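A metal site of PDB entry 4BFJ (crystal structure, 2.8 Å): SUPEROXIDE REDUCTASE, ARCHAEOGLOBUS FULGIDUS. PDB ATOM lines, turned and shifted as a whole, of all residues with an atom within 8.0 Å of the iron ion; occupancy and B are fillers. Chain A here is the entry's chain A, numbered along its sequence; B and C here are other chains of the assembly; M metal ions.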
ATOM      1  N   LYS A  10     -18.130  28.837 -34.057  1.00  0.00           N
ATOM      2  CA  LYS A  10     -17.297  29.085 -32.890  1.00  0.00           C
ATOM      3  C   LYS A  10     -17.700  28.194 -31.703  1.00  0.00           C
ATOM      4  O   LYS A  10     -16.823  27.685 -30.991  1.00  0.00           O
ATOM      5  CB  LYS A  10     -17.344  30.561 -32.460  1.00  0.00           C
ATOM      6  CG  LYS A  10     -16.853  31.597 -33.474  1.00  0.00           C
ATOM      7  CD  LYS A  10     -16.989  33.029 -32.939  1.00  0.00           C
ATOM      8  NZ  LYS A  10     -15.566  33.239 -30.714  1.00  0.00           N
ATOM      9  N   LYS A  13     -16.608  24.422 -32.231  1.00  0.00           N
ATOM     10  CA  LYS A  13     -15.154  24.306 -32.136  1.00  0.00           C
ATOM     11  C   LYS A  13     -14.719  23.980 -30.708  1.00  0.00           C
ATOM     12  O   LYS A  13     -13.682  23.363 -30.500  1.00  0.00           O
ATOM     13  CB  LYS A  13     -14.491  25.599 -32.613  1.00  0.00           C
ATOM     14  CG  LYS A  13     -12.990  25.524 -32.739  1.00  0.00           C
ATOM     15  CD  LYS A  13     -12.408  26.727 -33.467  1.00  0.00           C
ATOM     16  CE  LYS A  13     -12.737  28.049 -32.765  1.00  0.00           C
ATOM     17  NZ  LYS A  13     -11.913  29.178 -33.291  1.00  0.00           N
ATOM     18  N   HIS A  14     -15.548  24.367 -29.750  1.00  0.00           N
ATOM     19  CA  HIS A  14     -15.222  24.345 -28.333  1.00  0.00           C
ATOM     20  C   HIS A  14     -15.946  23.283 -27.524  1.00  0.00           C
ATOM     21  O   HIS A  14     -15.441  22.854 -26.491  1.00  0.00           O
ATOM     22  CB  HIS A  14     -15.542  25.691 -27.722  1.00  0.00           C
ATOM     23  CG  HIS A  14     -14.530  26.732 -28.016  1.00  0.00           C
ATOM     24  ND1 HIS A  14     -14.736  27.741 -28.921  1.00  0.00           N
ATOM     25  CD2 HIS A  14     -13.272  26.898 -27.549  1.00  0.00           C
ATOM     26  CE1 HIS A  14     -13.669  28.509 -28.976  1.00  0.00           C
ATOM     27  NE2 HIS A  14     -12.755  28.010 -28.160  1.00  0.00           N
ATOM     28  N   VAL A  34     -12.292  17.945 -27.816  1.00  0.00           N
ATOM     29  CA  VAL A  34     -12.669  19.290 -28.224  1.00  0.00           C
ATOM     30  C   VAL A  34     -12.010  19.620 -29.548  1.00  0.00           C
ATOM     31  O   VAL A  34     -10.799  19.540 -29.678  1.00  0.00           O
ATOM     32  CB  VAL A  34     -12.219  20.333 -27.172  1.00  0.00           C
ATOM     33  CG1 VAL A  34     -12.347  21.762 -27.713  1.00  0.00           C
ATOM     34  CG2 VAL A  34     -13.018  20.183 -25.906  1.00  0.00           C
ATOM     35  N   HIS A  40      -9.640  23.160 -33.185  1.00  0.00           N
ATOM     36  CA  HIS A  40      -9.335  24.290 -32.302  1.00  0.00           C
ATOM     37  C   HIS A  40      -7.817  24.480 -32.112  1.00  0.00           C
ATOM     38  O   HIS A  40      -7.090  23.526 -31.796  1.00  0.00           O
ATOM     39  CB  HIS A  40     -10.033  24.118 -30.945  1.00  0.00           C
ATOM     40  CG  HIS A  40      -9.836  25.275 -30.002  1.00  0.00           C
ATOM     41  ND1 HIS A  40      -8.674  25.487 -29.285  1.00  0.00           N
ATOM     42  CD2 HIS A  40     -10.696  26.251 -29.616  1.00  0.00           C
ATOM     43  CE1 HIS A  40      -8.820  26.553 -28.533  1.00  0.00           C
ATOM     44  NE2 HIS A  40     -10.040  27.030 -28.705  1.00  0.00           N
ATOM     45  N   PRO A  41      -7.355  25.730 -32.287  1.00  0.00           N
ATOM     46  CA  PRO A  41      -5.941  26.121 -32.176  1.00  0.00           C
ATOM     47  C   PRO A  41      -5.260  25.487 -30.971  1.00  0.00           C
ATOM     48  O   PRO A  41      -5.872  25.377 -29.914  1.00  0.00           O
ATOM     49  CB  PRO A  41      -6.035  27.633 -31.989  1.00  0.00           C
ATOM     50  CG  PRO A  41      -7.234  28.011 -32.771  1.00  0.00           C
ATOM     51  CD  PRO A  41      -8.219  26.897 -32.567  1.00  0.00           C
ATOM     52  N   HIS A  46      -3.020  30.236 -27.213  1.00  0.00           N
ATOM     53  CA  HIS A  46      -4.438  29.887 -27.329  1.00  0.00           C
ATOM     54  C   HIS A  46      -4.618  28.370 -27.527  1.00  0.00           C
ATOM     55  O   HIS A  46      -4.135  27.820 -28.510  1.00  0.00           O
ATOM     56  CB  HIS A  46      -5.023  30.647 -28.511  1.00  0.00           C
ATOM     57  CG  HIS A  46      -6.463  30.344 -28.802  1.00  0.00           C
ATOM     58  ND1 HIS A  46      -7.078  30.685 -29.993  1.00  0.00           N
ATOM     59  CD2 HIS A  46      -7.418  29.741 -28.047  1.00  0.00           C
ATOM     60  CE1 HIS A  46      -8.339  30.305 -29.954  1.00  0.00           C
ATOM     61  NE2 HIS A  46      -8.573  29.727 -28.790  1.00  0.00           N
ATOM     62  N   HIS A  47      -5.303  27.714 -26.597  1.00  0.00           N
ATOM     63  CA  HIS A  47      -5.329  26.241 -26.568  1.00  0.00           C
ATOM     64  C   HIS A  47      -6.338  25.741 -25.530  1.00  0.00           C
ATOM     65  O   HIS A  47      -6.801  26.504 -24.686  1.00  0.00           O
ATOM     66  CB  HIS A  47      -3.933  25.750 -26.185  1.00  0.00           C
ATOM     67  CG  HIS A  47      -3.440  26.341 -24.900  1.00  0.00           C
ATOM     68  ND1 HIS A  47      -2.642  27.470 -24.856  1.00  0.00           N
ATOM     69  CD2 HIS A  47      -3.704  26.019 -23.618  1.00  0.00           C
ATOM     70  CE1 HIS A  47      -2.412  27.790 -23.599  1.00  0.00           C
ATOM     71  NE2 HIS A  47      -3.049  26.932 -22.829  1.00  0.00           N
ATOM     72  N   ILE A  48      -6.664  24.453 -25.577  1.00  0.00           N
ATOM     73  CA  ILE A  48      -7.582  23.839 -24.605  1.00  0.00           C
ATOM     74  C   ILE A  48      -6.828  23.258 -23.430  1.00  0.00           C
ATOM     75  O   ILE A  48      -5.924  22.425 -23.578  1.00  0.00           O
ATOM     76  CB  ILE A  48      -8.447  22.728 -25.234  1.00  0.00           C
ATOM     77  CG1 ILE A  48      -9.240  23.287 -26.436  1.00  0.00           C
ATOM     78  CG2 ILE A  48      -9.359  22.064 -24.204  1.00  0.00           C
ATOM     79  CD1 ILE A  48     -10.021  24.525 -26.125  1.00  0.00           C
ATOM     80  N   TYR A 109     -12.061  23.683 -21.018  1.00  0.00           N
ATOM     81  CA  TYR A 109     -11.660  25.067 -20.838  1.00  0.00           C
ATOM     82  C   TYR A 109     -10.712  25.563 -21.910  1.00  0.00           C
ATOM     83  O   TYR A 109      -9.698  24.938 -22.185  1.00  0.00           O
ATOM     84  CB  TYR A 109     -11.050  25.231 -19.451  1.00  0.00           C
ATOM     85  CG  TYR A 109     -10.579  26.632 -19.127  1.00  0.00           C
ATOM     86  CD1 TYR A 109     -11.475  27.689 -19.083  1.00  0.00           C
ATOM     87  CD2 TYR A 109      -9.238  26.887 -18.859  1.00  0.00           C
ATOM     88  CE1 TYR A 109     -11.056  28.976 -18.780  1.00  0.00           C
ATOM     89  CE2 TYR A 109      -8.806  28.168 -18.554  1.00  0.00           C
ATOM     90  CZ  TYR A 109      -9.712  29.203 -18.508  1.00  0.00           C
ATOM     91  OH  TYR A 109      -9.290  30.460 -18.218  1.00  0.00           O
ATOM     92  N   CYS A 110     -11.064  26.683 -22.528  1.00  0.00           N
ATOM     93  CA  CYS A 110     -10.158  27.385 -23.418  1.00  0.00           C
ATOM     94  C   CYS A 110      -9.549  28.504 -22.615  1.00  0.00           C
ATOM     95  O   CYS A 110     -10.237  29.160 -21.826  1.00  0.00           O
ATOM     96  CB  CYS A 110     -10.904  27.966 -24.605  1.00  0.00           C
ATOM     97  SG  CYS A 110      -9.878  28.851 -25.821  1.00  0.00           S
ATOM     98  N   ASN A 111      -8.254  28.752 -22.811  1.00  0.00           N
ATOM     99  CA  ASN A 111      -7.580  29.773 -22.025  1.00  0.00           C
ATOM    100  C   ASN A 111      -8.013  31.207 -22.375  1.00  0.00           C
ATOM    101  O   ASN A 111      -7.685  32.146 -21.653  1.00  0.00           O
ATOM    102  CB  ASN A 111      -6.060  29.625 -22.123  1.00  0.00           C
ATOM    103  CG  ASN A 111      -5.534  29.927 -23.514  1.00  0.00           C
ATOM    104  OD1 ASN A 111      -6.207  29.656 -24.532  1.00  0.00           O
ATOM    105  ND2 ASN A 111      -4.327  30.507 -23.579  1.00  0.00           N
ATOM    106  N   ILE A 112      -8.738  31.372 -23.467  1.00  0.00           N
ATOM    107  CA  ILE A 112      -9.253  32.696 -23.831  1.00  0.00           C
ATOM    108  C   ILE A 112     -10.750  32.673 -24.129  1.00  0.00           C
ATOM    109  O   ILE A 112     -11.376  33.730 -24.156  1.00  0.00           O
ATOM    110  CB  ILE A 112      -8.522  33.309 -25.064  1.00  0.00           C
ATOM    111  CG1 ILE A 112      -8.948  32.608 -26.364  1.00  0.00           C
ATOM    112  CG2 ILE A 112      -7.018  33.281 -24.887  1.00  0.00           C
ATOM    113  CD1 ILE A 112      -8.344  33.200 -27.624  1.00  0.00           C
ATOM    114  N   HIS A 113     -11.322  31.501 -24.384  1.00  0.00           N
ATOM    115  CA  HIS A 113     -12.742  31.417 -24.762  1.00  0.00           C
ATOM    116  C   HIS A 113     -13.661  30.739 -23.735  1.00  0.00           C
ATOM    117  O   HIS A 113     -14.724  30.232 -24.093  1.00  0.00           O
ATOM    118  CB  HIS A 113     -12.927  30.722 -26.127  1.00  0.00           C
ATOM    119  CG  HIS A 113     -12.319  31.472 -27.273  1.00  0.00           C
ATOM    120  ND1 HIS A 113     -11.405  30.892 -28.124  1.00  0.00           N
ATOM    121  CD2 HIS A 113     -12.502  32.744 -27.712  1.00  0.00           C
ATOM    122  CE1 HIS A 113     -11.052  31.777 -29.043  1.00  0.00           C
ATOM    123  NE2 HIS A 113     -11.698  32.909 -28.811  1.00  0.00           N
ATOM    124  N   GLY A 114     -13.251  30.725 -22.476  1.00  0.00           N
ATOM    125  CA  GLY A 114     -14.125  30.373 -21.387  1.00  0.00           C
ATOM    126  C   GLY A 114     -14.369  28.893 -21.148  1.00  0.00           C
ATOM    127  O   GLY A 114     -13.738  28.022 -21.727  1.00  0.00           O
ATOM    128  N   TRP A 116     -16.875  25.405 -20.866  1.00  0.00           N
ATOM    129  CA  TRP A 116     -17.713  24.731 -21.842  1.00  0.00           C
ATOM    130  C   TRP A 116     -18.293  23.441 -21.289  1.00  0.00           C
ATOM    131  O   TRP A 116     -17.688  22.777 -20.482  1.00  0.00           O
ATOM    132  CB  TRP A 116     -16.927  24.476 -23.126  1.00  0.00           C
ATOM    133  CG  TRP A 116     -16.601  25.749 -23.857  1.00  0.00           C
ATOM    134  CD1 TRP A 116     -15.544  26.566 -23.644  1.00  0.00           C
ATOM    135  CD2 TRP A 116     -17.385  26.353 -24.890  1.00  0.00           C
ATOM    136  NE1 TRP A 116     -15.609  27.655 -24.473  1.00  0.00           N
ATOM    137  CE2 TRP A 116     -16.724  27.554 -25.250  1.00  0.00           C
ATOM    138  CE3 TRP A 116     -18.573  26.026 -25.539  1.00  0.00           C
ATOM    139  CZ2 TRP A 116     -17.209  28.405 -26.246  1.00  0.00           C
ATOM    140  CZ3 TRP A 116     -19.048  26.867 -26.510  1.00  0.00           C
ATOM    141  CH2 TRP A 116     -18.369  28.042 -26.856  1.00  0.00           C
ATOM    142  N   VAL B  78      -8.569  37.027 -25.892  1.00  0.00           N
ATOM    143  CA  VAL B  78      -8.900  37.055 -27.322  1.00  0.00           C
ATOM    144  C   VAL B  78      -8.143  38.182 -28.034  1.00  0.00           C
ATOM    145  O   VAL B  78      -8.028  38.192 -29.253  1.00  0.00           O
ATOM    146  CB  VAL B  78     -10.423  37.237 -27.566  1.00  0.00           C
ATOM    147  CG1 VAL B  78     -11.216  36.082 -26.989  1.00  0.00           C
ATOM    148  CG2 VAL B  78     -10.918  38.558 -26.981  1.00  0.00           C
ATOM    149  N   PHE C  62     -15.206  36.797 -21.723  1.00  0.00           N
ATOM    150  CA  PHE C  62     -15.000  35.453 -21.192  1.00  0.00           C
ATOM    151  C   PHE C  62     -14.426  35.424 -19.774  1.00  0.00           C
ATOM    152  O   PHE C  62     -13.710  36.337 -19.358  1.00  0.00           O
ATOM    153  CB  PHE C  62     -14.116  34.643 -22.136  1.00  0.00           C
ATOM    154  CG  PHE C  62     -14.678  34.500 -23.508  1.00  0.00           C
ATOM    155  CD1 PHE C  62     -15.645  33.534 -23.777  1.00  0.00           C
ATOM    156  CD2 PHE C  62     -14.286  35.354 -24.528  1.00  0.00           C
ATOM    157  CE1 PHE C  62     -16.171  33.416 -25.031  1.00  0.00           C
ATOM    158  CE2 PHE C  62     -14.828  35.234 -25.793  1.00  0.00           C
ATOM    159  CZ  PHE C  62     -15.771  34.272 -26.045  1.00  0.00           C
HETATM  160 FE    FE M   1     -10.805  28.968 -28.083  1.00  0.00          FE
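ND1 of His 113 is bound to the iron ion.
NE2 of His 14 is bound to the iron ion, 2.2 Å away.
A ring nitrogen (NE2) of His 40 binds the iron ion (2.2 Å).
SG of Cys 110 binds the iron ion (2.4 Å).
The iron ion is bound by NE2 of His 46, at 2.5 Å.
The iron ion has five donor atoms within binding distance.
Within 4 Å of the iron ion: His 14, His 40, His 46, Cys 110 and His 113.
The backbone carbonyl oxygen (O) of His 113 lies within hydrogen-bond range of the indole nitrogen (NE1) of Trp 116 (2.8 Å).
O of Lys 10 is in hydrogen-bond range of ND1 of His 14.
The backbone NH (N) of Ile 112 sits close to the side-chain sulfur (SG) of Cys 110 (3.6 Å).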
